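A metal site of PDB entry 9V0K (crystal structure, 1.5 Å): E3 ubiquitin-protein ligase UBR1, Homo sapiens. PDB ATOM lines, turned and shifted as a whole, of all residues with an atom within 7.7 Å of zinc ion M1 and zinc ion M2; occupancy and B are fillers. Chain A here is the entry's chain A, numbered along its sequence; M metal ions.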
ATOM      1  N   GLN A   3      24.137   4.297   4.335  1.00  0.00           N
ATOM      2  CA  GLN A   3      24.098   3.149   3.455  1.00  0.00           C
ATOM      3  C   GLN A   3      22.720   3.031   2.831  1.00  0.00           C
ATOM      4  O   GLN A   3      21.717   3.375   3.444  1.00  0.00           O
ATOM      5  CB  GLN A   3      24.338   1.842   4.219  1.00  0.00           C
ATOM      6  CG  GLN A   3      25.722   1.630   4.770  1.00  0.00           C
ATOM      7  CD  GLN A   3      25.775   0.433   5.698  1.00  0.00           C
ATOM      8  OE1 GLN A   3      24.909   0.266   6.556  1.00  0.00           O
ATOM      9  NE2 GLN A   3      26.776  -0.420   5.500  1.00  0.00           N
ATOM     10  N   LEU A   4      22.681   2.440   1.636  1.00  0.00           N
ATOM     11  CA  LEU A   4      21.435   2.010   1.037  1.00  0.00           C
ATOM     12  C   LEU A   4      21.166   0.555   1.406  1.00  0.00           C
ATOM     13  O   LEU A   4      22.074  -0.276   1.348  1.00  0.00           O
ATOM     14  CB  LEU A   4      21.488   2.106  -0.486  1.00  0.00           C
ATOM     15  CG  LEU A   4      21.382   3.483  -1.123  1.00  0.00           C
ATOM     16  CD1 LEU A   4      21.937   3.376  -2.530  1.00  0.00           C
ATOM     17  CD2 LEU A   4      19.967   4.004  -1.176  1.00  0.00           C
ATOM     18  N   CYS A   5      19.914   0.252   1.723  1.00  0.00           N
ATOM     19  CA  CYS A   5      19.562  -1.138   2.031  1.00  0.00           C
ATOM     20  C   CYS A   5      19.690  -2.020   0.794  1.00  0.00           C
ATOM     21  O   CYS A   5      20.386  -3.034   0.811  1.00  0.00           O
ATOM     22  CB  CYS A   5      18.138  -1.227   2.588  1.00  0.00           C
ATOM     23  SG  CYS A   5      17.611  -2.941   2.741  1.00  0.00           S
ATOM     24  N   GLY A   6      18.949  -1.676  -0.260  1.00  0.00           N
ATOM     25  CA  GLY A   6      18.975  -2.374  -1.526  1.00  0.00           C
ATOM     26  C   GLY A   6      18.316  -3.738  -1.575  1.00  0.00           C
ATOM     27  O   GLY A   6      18.419  -4.399  -2.613  1.00  0.00           O
ATOM     28  N   ARG A   7      17.632  -4.170  -0.513  1.00  0.00           N
ATOM     29  CA  ARG A   7      17.060  -5.509  -0.487  1.00  0.00           C
ATOM     30  C   ARG A   7      16.052  -5.668  -1.621  1.00  0.00           C
ATOM     31  O   ARG A   7      15.221  -4.791  -1.852  1.00  0.00           O
ATOM     32  CB  ARG A   7      16.392  -5.825   0.865  1.00  0.00           C
ATOM     33  CG  ARG A   7      15.800  -7.239   0.903  1.00  0.00           C
ATOM     34  CD  ARG A   7      14.961  -7.534   2.156  1.00  0.00           C
ATOM     35  NE  ARG A   7      14.207  -8.760   1.964  1.00  0.00           N
ATOM     36  CZ  ARG A   7      14.761  -9.944   1.807  1.00  0.00           C
ATOM     37  NH1 ARG A   7      16.055 -10.142   2.005  1.00  0.00           N
ATOM     38  NH2 ARG A   7      14.000 -10.979   1.443  1.00  0.00           N
ATOM     39  N   VAL A   8      16.150  -6.782  -2.339  1.00  0.00           N
ATOM     40  CA  VAL A   8      15.186  -7.138  -3.378  1.00  0.00           C
ATOM     41  C   VAL A   8      14.209  -8.140  -2.787  1.00  0.00           C
ATOM     42  O   VAL A   8      14.606  -9.178  -2.236  1.00  0.00           O
ATOM     43  CB  VAL A   8      15.891  -7.708  -4.622  1.00  0.00           C
ATOM     44  CG1 VAL A   8      14.898  -8.231  -5.603  1.00  0.00           C
ATOM     45  CG2 VAL A   8      16.744  -6.624  -5.314  1.00  0.00           C
ATOM     46  N   PHE A   9      12.915  -7.829  -2.899  1.00  0.00           N
ATOM     47  CA  PHE A   9      11.889  -8.604  -2.213  1.00  0.00           C
ATOM     48  C   PHE A   9      11.689  -9.956  -2.880  1.00  0.00           C
ATOM     49  O   PHE A   9      11.813 -10.111  -4.099  1.00  0.00           O
ATOM     50  CB  PHE A   9      10.569  -7.833  -2.212  1.00  0.00           C
ATOM     51  CG  PHE A   9      10.667  -6.461  -1.596  1.00  0.00           C
ATOM     52  CD1 PHE A   9      11.087  -6.282  -0.290  1.00  0.00           C
ATOM     53  CD2 PHE A   9      10.321  -5.351  -2.333  1.00  0.00           C
ATOM     54  CE1 PHE A   9      11.182  -5.001   0.257  1.00  0.00           C
ATOM     55  CE2 PHE A   9      10.382  -4.087  -1.805  1.00  0.00           C
ATOM     56  CZ  PHE A   9      10.831  -3.909  -0.493  1.00  0.00           C
ATOM     57  N   VAL A  28       8.916   2.252  -0.809  1.00  0.00           N
ATOM     58  CA  VAL A  28       8.607   1.100   0.030  1.00  0.00           C
ATOM     59  C   VAL A  28       9.821   0.713   0.856  1.00  0.00           C
ATOM     60  O   VAL A  28      10.959   1.044   0.521  1.00  0.00           O
ATOM     61  CB  VAL A  28       8.117  -0.071  -0.855  1.00  0.00           C
ATOM     62  CG1 VAL A  28       9.177  -0.446  -1.902  1.00  0.00           C
ATOM     63  CG2 VAL A  28       7.732  -1.247  -0.032  1.00  0.00           C
ATOM     64  N   LEU A  29       9.574   0.011   1.972  1.00  0.00           N
ATOM     65  CA  LEU A  29      10.620  -0.456   2.850  1.00  0.00           C
ATOM     66  C   LEU A  29      10.464  -1.949   3.101  1.00  0.00           C
ATOM     67  O   LEU A  29       9.348  -2.459   3.116  1.00  0.00           O
ATOM     68  CB  LEU A  29      10.593   0.254   4.228  1.00  0.00           C
ATOM     69  CG  LEU A  29      10.782   1.772   4.168  1.00  0.00           C
ATOM     70  CD1 LEU A  29      10.328   2.385   5.477  1.00  0.00           C
ATOM     71  CD2 LEU A  29      12.251   2.110   3.932  1.00  0.00           C
ATOM     72  N   CYS A  30      11.603  -2.629   3.312  1.00  0.00           N
ATOM     73  CA  CYS A  30      11.579  -3.987   3.814  1.00  0.00           C
ATOM     74  C   CYS A  30      11.209  -3.985   5.290  1.00  0.00           C
ATOM     75  O   CYS A  30      11.285  -2.967   5.973  1.00  0.00           O
ATOM     76  CB  CYS A  30      12.928  -4.690   3.616  1.00  0.00           C
ATOM     77  SG  CYS A  30      14.308  -4.149   4.691  1.00  0.00           S
ATOM     78  N   MET A  31      10.771  -5.142   5.771  1.00  0.00           N
ATOM     79  CA  MET A  31      10.360  -5.231   7.162  1.00  0.00           C
ATOM     80  C   MET A  31      11.466  -4.786   8.122  1.00  0.00           C
ATOM     81  O   MET A  31      11.198  -4.021   9.059  1.00  0.00           O
ATOM     82  CB  MET A  31       9.923  -6.651   7.505  1.00  0.00           C
ATOM     83  CG  MET A  31       9.143  -6.625   8.797  1.00  0.00           C
ATOM     84  SD  MET A  31      10.272  -7.101  10.136  1.00  0.00           S
ATOM     85  CE  MET A  31      10.998  -8.660   9.552  1.00  0.00           C
ATOM     86  N   ASP A  32      12.682  -5.308   7.950  1.00  0.00           N
ATOM     87  CA  ASP A  32      13.765  -4.984   8.875  1.00  0.00           C
ATOM     88  C   ASP A  32      13.965  -3.485   8.990  1.00  0.00           C
ATOM     89  O   ASP A  32      14.076  -2.941  10.095  1.00  0.00           O
ATOM     90  CB  ASP A  32      15.062  -5.646   8.400  1.00  0.00           C
ATOM     91  CG  ASP A  32      15.131  -7.098   8.759  1.00  0.00           C
ATOM     92  OD1 ASP A  32      14.600  -7.918   7.997  1.00  0.00           O
ATOM     93  OD2 ASP A  32      15.749  -7.399   9.809  1.00  0.00           O
ATOM     94  N   CYS A  33      14.009  -2.788   7.851  1.00  0.00           N
ATOM     95  CA  CYS A  33      14.205  -1.349   7.869  1.00  0.00           C
ATOM     96  C   CYS A  33      12.990  -0.644   8.474  1.00  0.00           C
ATOM     97  O   CYS A  33      13.142   0.257   9.293  1.00  0.00           O
ATOM     98  CB  CYS A  33      14.485  -0.842   6.444  1.00  0.00           C
ATOM     99  SG  CYS A  33      16.129  -1.385   5.816  1.00  0.00           S
ATOM    100  N   PHE A  34      11.778  -1.055   8.074  1.00  0.00           N
ATOM    101  CA  PHE A  34      10.563  -0.427   8.582  1.00  0.00           C
ATOM    102  C   PHE A  34      10.525  -0.449  10.106  1.00  0.00           C
ATOM    103  O   PHE A  34      10.303   0.594  10.733  1.00  0.00           O
ATOM    104  CB  PHE A  34       9.341  -1.116   7.959  1.00  0.00           C
ATOM    105  CG  PHE A  34       8.063  -0.758   8.582  1.00  0.00           C
ATOM    106  CD1 PHE A  34       7.426   0.430   8.263  1.00  0.00           C
ATOM    107  CD2 PHE A  34       7.448  -1.634   9.482  1.00  0.00           C
ATOM    108  CE1 PHE A  34       6.202   0.747   8.842  1.00  0.00           C
ATOM    109  CE2 PHE A  34       6.236  -1.313  10.035  1.00  0.00           C
ATOM    110  CZ  PHE A  34       5.615  -0.129   9.723  1.00  0.00           C
ATOM    111  N   ASP A  36      12.816  -0.636  12.197  1.00  0.00           N
ATOM    112  CA  ASP A  36      13.921   0.122  12.783  1.00  0.00           C
ATOM    113  C   ASP A  36      13.893   1.581  12.318  1.00  0.00           C
ATOM    114  O   ASP A  36      14.929   2.251  12.304  1.00  0.00           O
ATOM    115  CB  ASP A  36      15.255  -0.528  12.437  1.00  0.00           C
ATOM    116  CG  ASP A  36      15.765  -1.474  13.530  1.00  0.00           C
ATOM    117  OD1 ASP A  36      15.266  -1.431  14.671  1.00  0.00           O
ATOM    118  OD2 ASP A  36      16.676  -2.274  13.228  1.00  0.00           O
ATOM    119  N   SER A  37      12.717   2.074  11.948  1.00  0.00           N
ATOM    120  CA  SER A  37      12.559   3.409  11.367  1.00  0.00           C
ATOM    121  C   SER A  37      11.409   4.141  12.028  1.00  0.00           C
ATOM    122  O   SER A  37      10.569   3.570  12.725  1.00  0.00           O
ATOM    123  CB  SER A  37      12.303   3.337   9.836  1.00  0.00           C
ATOM    124  OG  SER A  37      10.920   3.017   9.582  1.00  0.00           O
ATOM    125  N   PHE A  54      12.303  -3.381  -4.684  1.00  0.00           N
ATOM    126  CA  PHE A  54      13.404  -3.219  -3.734  1.00  0.00           C
ATOM    127  C   PHE A  54      13.103  -2.178  -2.657  1.00  0.00           C
ATOM    128  O   PHE A  54      12.316  -1.248  -2.844  1.00  0.00           O
ATOM    129  CB  PHE A  54      14.702  -2.849  -4.483  1.00  0.00           C
ATOM    130  CG  PHE A  54      14.548  -1.637  -5.377  1.00  0.00           C
ATOM    131  CD1 PHE A  54      14.116  -1.783  -6.669  1.00  0.00           C
ATOM    132  CD2 PHE A  54      14.856  -0.372  -4.915  1.00  0.00           C
ATOM    133  CE1 PHE A  54      13.977  -0.691  -7.478  1.00  0.00           C
ATOM    134  CE2 PHE A  54      14.714   0.727  -5.732  1.00  0.00           C
ATOM    135  CZ  PHE A  54      14.251   0.568  -7.001  1.00  0.00           C
ATOM    136  N   CYS A  55      13.781  -2.343  -1.529  1.00  0.00           N
ATOM    137  CA  CYS A  55      13.668  -1.430  -0.399  1.00  0.00           C
ATOM    138  C   CYS A  55      14.326  -0.106  -0.725  1.00  0.00           C
ATOM    139  O   CYS A  55      15.433  -0.088  -1.265  1.00  0.00           O
ATOM    140  CB  CYS A  55      14.338  -2.059   0.811  1.00  0.00           C
ATOM    141  SG  CYS A  55      14.383  -1.030   2.288  1.00  0.00           S
ATOM    142  N   ASP A  56      13.644   1.011  -0.423  1.00  0.00           N
ATOM    143  CA  ASP A  56      14.148   2.365  -0.627  1.00  0.00           C
ATOM    144  C   ASP A  56      14.812   2.985   0.616  1.00  0.00           C
ATOM    145  O   ASP A  56      15.108   4.190   0.626  1.00  0.00           O
ATOM    146  CB  ASP A  56      12.999   3.256  -1.096  1.00  0.00           C
ATOM    147  CG  ASP A  56      12.428   2.818  -2.452  1.00  0.00           C
ATOM    148  OD1 ASP A  56      13.227   2.643  -3.402  1.00  0.00           O
ATOM    149  OD2 ASP A  56      11.210   2.614  -2.553  1.00  0.00           O
ATOM    150  N   CYS A  57      15.077   2.209   1.651  1.00  0.00           N
ATOM    151  CA  CYS A  57      15.799   2.745   2.792  1.00  0.00           C
ATOM    152  C   CYS A  57      17.184   3.229   2.380  1.00  0.00           C
ATOM    153  O   CYS A  57      17.937   2.501   1.733  1.00  0.00           O
ATOM    154  CB  CYS A  57      15.926   1.688   3.874  1.00  0.00           C
ATOM    155  SG  CYS A  57      16.782   2.338   5.328  1.00  0.00           S
ATOM    156  N   GLY A  58      17.535   4.440   2.815  1.00  0.00           N
ATOM    157  CA  GLY A  58      18.790   5.052   2.440  1.00  0.00           C
ATOM    158  C   GLY A  58      18.719   5.959   1.245  1.00  0.00           C
ATOM    159  O   GLY A  58      19.688   6.679   0.964  1.00  0.00           O
ATOM    160  N   PRO A  67      14.726   9.098   5.985  1.00  0.00           N
ATOM    161  CA  PRO A  67      15.158   8.260   4.854  1.00  0.00           C
ATOM    162  C   PRO A  67      15.986   7.061   5.275  1.00  0.00           C
ATOM    163  O   PRO A  67      16.109   6.126   4.483  1.00  0.00           O
ATOM    164  CB  PRO A  67      15.968   9.229   3.994  1.00  0.00           C
ATOM    165  CG  PRO A  67      16.482  10.234   4.977  1.00  0.00           C
ATOM    166  CD  PRO A  67      15.358  10.425   5.961  1.00  0.00           C
ATOM    167  N   PHE A  68      16.558   7.037   6.482  1.00  0.00           N
ATOM    168  CA  PHE A  68      17.364   5.926   6.936  1.00  0.00           C
ATOM    169  C   PHE A  68      16.745   5.296   8.166  1.00  0.00           C
ATOM    170  O   PHE A  68      16.334   6.007   9.093  1.00  0.00           O
ATOM    171  CB  PHE A  68      18.808   6.351   7.296  1.00  0.00           C
ATOM    172  CG  PHE A  68      19.577   6.961   6.172  1.00  0.00           C
ATOM    173  CD1 PHE A  68      20.355   6.177   5.348  1.00  0.00           C
ATOM    174  CD2 PHE A  68      19.538   8.317   5.962  1.00  0.00           C
ATOM    175  CE1 PHE A  68      21.068   6.742   4.318  1.00  0.00           C
ATOM    176  CE2 PHE A  68      20.263   8.891   4.922  1.00  0.00           C
ATOM    177  CZ  PHE A  68      21.008   8.094   4.097  1.00  0.00           C
ATOM    178  N   CYS A  69      16.742   3.971   8.204  1.00  0.00           N
ATOM    179  CA  CYS A  69      16.515   3.259   9.461  1.00  0.00           C
ATOM    180  C   CYS A  69      17.784   3.292  10.314  1.00  0.00           C
ATOM    181  O   CYS A  69      18.838   3.769   9.906  1.00  0.00           O
ATOM    182  CB  CYS A  69      16.095   1.823   9.175  1.00  0.00           C
ATOM    183  SG  CYS A  69      17.456   0.743   8.712  1.00  0.00           S
ATOM    184  N   VAL A  70      17.683   2.786  11.547  1.00  0.00           N
ATOM    185  CA  VAL A  70      18.821   2.963  12.462  1.00  0.00           C
ATOM    186  C   VAL A  70      19.980   2.041  12.100  1.00  0.00           C
ATOM    187  O   VAL A  70      21.094   2.221  12.628  1.00  0.00           O
ATOM    188  CB  VAL A  70      18.403   2.792  13.932  1.00  0.00           C
ATOM    189  CG1 VAL A  70      17.417   3.884  14.334  1.00  0.00           C
ATOM    190  CG2 VAL A  70      17.842   1.424  14.202  1.00  0.00           C
ATOM    191  N   ASN A  71      19.781   1.093  11.206  1.00  0.00           N
ATOM    192  CA  ASN A  71      20.841   0.205  10.764  1.00  0.00           C
ATOM    193  C   ASN A  71      21.602   0.752   9.580  1.00  0.00           C
ATOM    194  O   ASN A  71      22.782   0.418   9.394  1.00  0.00           O
ATOM    195  CB  ASN A  71      20.245  -1.161  10.430  1.00  0.00           C
ATOM    196  CG  ASN A  71      19.498  -1.747  11.607  1.00  0.00           C
ATOM    197  OD1 ASN A  71      20.009  -1.794  12.721  1.00  0.00           O
ATOM    198  ND2 ASN A  71      18.253  -2.137  11.383  1.00  0.00           N
ATOM    199  N   HIS A  72      20.975   1.613   8.806  1.00  0.00           N
ATOM    200  CA  HIS A  72      21.581   2.168   7.600  1.00  0.00           C
ATOM    201  C   HIS A  72      21.967   3.631   7.709  1.00  0.00           C
ATOM    202  O   HIS A  72      22.707   4.122   6.845  1.00  0.00           O
ATOM    203  CB  HIS A  72      20.618   1.943   6.430  1.00  0.00           C
ATOM    204  CG  HIS A  72      20.520   0.518   6.042  1.00  0.00           C
ATOM    205  ND1 HIS A  72      19.328  -0.175   6.036  1.00  0.00           N
ATOM    206  CD2 HIS A  72      21.469  -0.366   5.668  1.00  0.00           C
ATOM    207  CE1 HIS A  72      19.552  -1.425   5.671  1.00  0.00           C
ATOM    208  NE2 HIS A  72      20.853  -1.571   5.449  1.00  0.00           N
ATOM    209  N   GLU A  73      21.543   4.321   8.776  1.00  0.00           N
ATOM    210  CA  GLU A  73      22.079   5.628   9.129  1.00  0.00           C
ATOM    211  C   GLU A  73      23.619   5.610   9.206  1.00  0.00           C
ATOM    212  O   GLU A  73      24.249   6.496   8.604  1.00  0.00           O
ATOM    213  CB  GLU A  73      21.518   6.095  10.480  1.00  0.00           C
ATOM    214  CG  GLU A  73      21.499   7.608  10.692  1.00  0.00           C
ATOM    215  CD  GLU A  73      20.480   8.337   9.853  1.00  0.00           C
ATOM    216  OE1 GLU A  73      20.881   9.064   8.913  1.00  0.00           O
ATOM    217  OE2 GLU A  73      19.263   8.167  10.111  1.00  0.00           O
HETATM  218 ZN    ZN M   1      15.551  -2.409   3.734  1.00  0.00          ZN
HETATM  219 ZN    ZN M   2      17.440   0.454   6.439  1.00  0.00          ZN
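SG of Cys 55 is bound to zinc ion M1, at 2.3 Å.
Zinc ion M1 is bound by the side-chain sulfur (SG) of Cys 30, 2.3 Å away.
Zinc ion M1 is bound by SG of Cys 5, 2.3 Å away.
Zinc ion M1 is bound by SG of Cys 33 (2.4 Å).
Zinc ion M1 has four donor atoms within binding distance.
The backbone NH (N) of Gln 3 sits at hydrogen-bond distance from the backbone carbonyl oxygen (O) of His 72, 2.9 Å away.
The side-chain sulfur (SG) of Cys 55 lies close to the backbone NH (N) of Cys 57 (3.4 Å).
The backbone NH of Cys 5 lies within hydrogen-bond range of the backbone carbonyl oxygen of Cys 57, 3.0 Å away.
The side-chain sulfur of Cys 69 lies close to the backbone NH of Asn 71 (3.4 Å).
The backbone NH (N) of Cys 55 is in hydrogen-bond range of the backbone carbonyl oxygen (O) of Arg 7 (2.9 Å).
The side-chain sulfur (SG) of Cys 5 sits close to the backbone NH (N) of Arg 7 (3.5 Å).
Zinc ion M2 is bound by a ring nitrogen (ND1) of His 72 (2.0 Å), the side-chain sulfur (SG) of Cys 57 (2.3 Å), the side-chain sulfur (SG) of Cys 69 (2.3 Å) and the side-chain sulfur (SG) of Cys 33 (2.3 Å).
Zinc ion M2 has four donor atoms within binding distance.
Four residues have an atom within 4 Å of zinc ion M2: Cys 33, Cys 57, Cys 69 and His 72.
Of the 28 residues printed, 4 come within 4 Å of zinc ion M1.
The nearest printed residue that does not touch zinc ion M1 is Cys 57 (4.1 Å).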
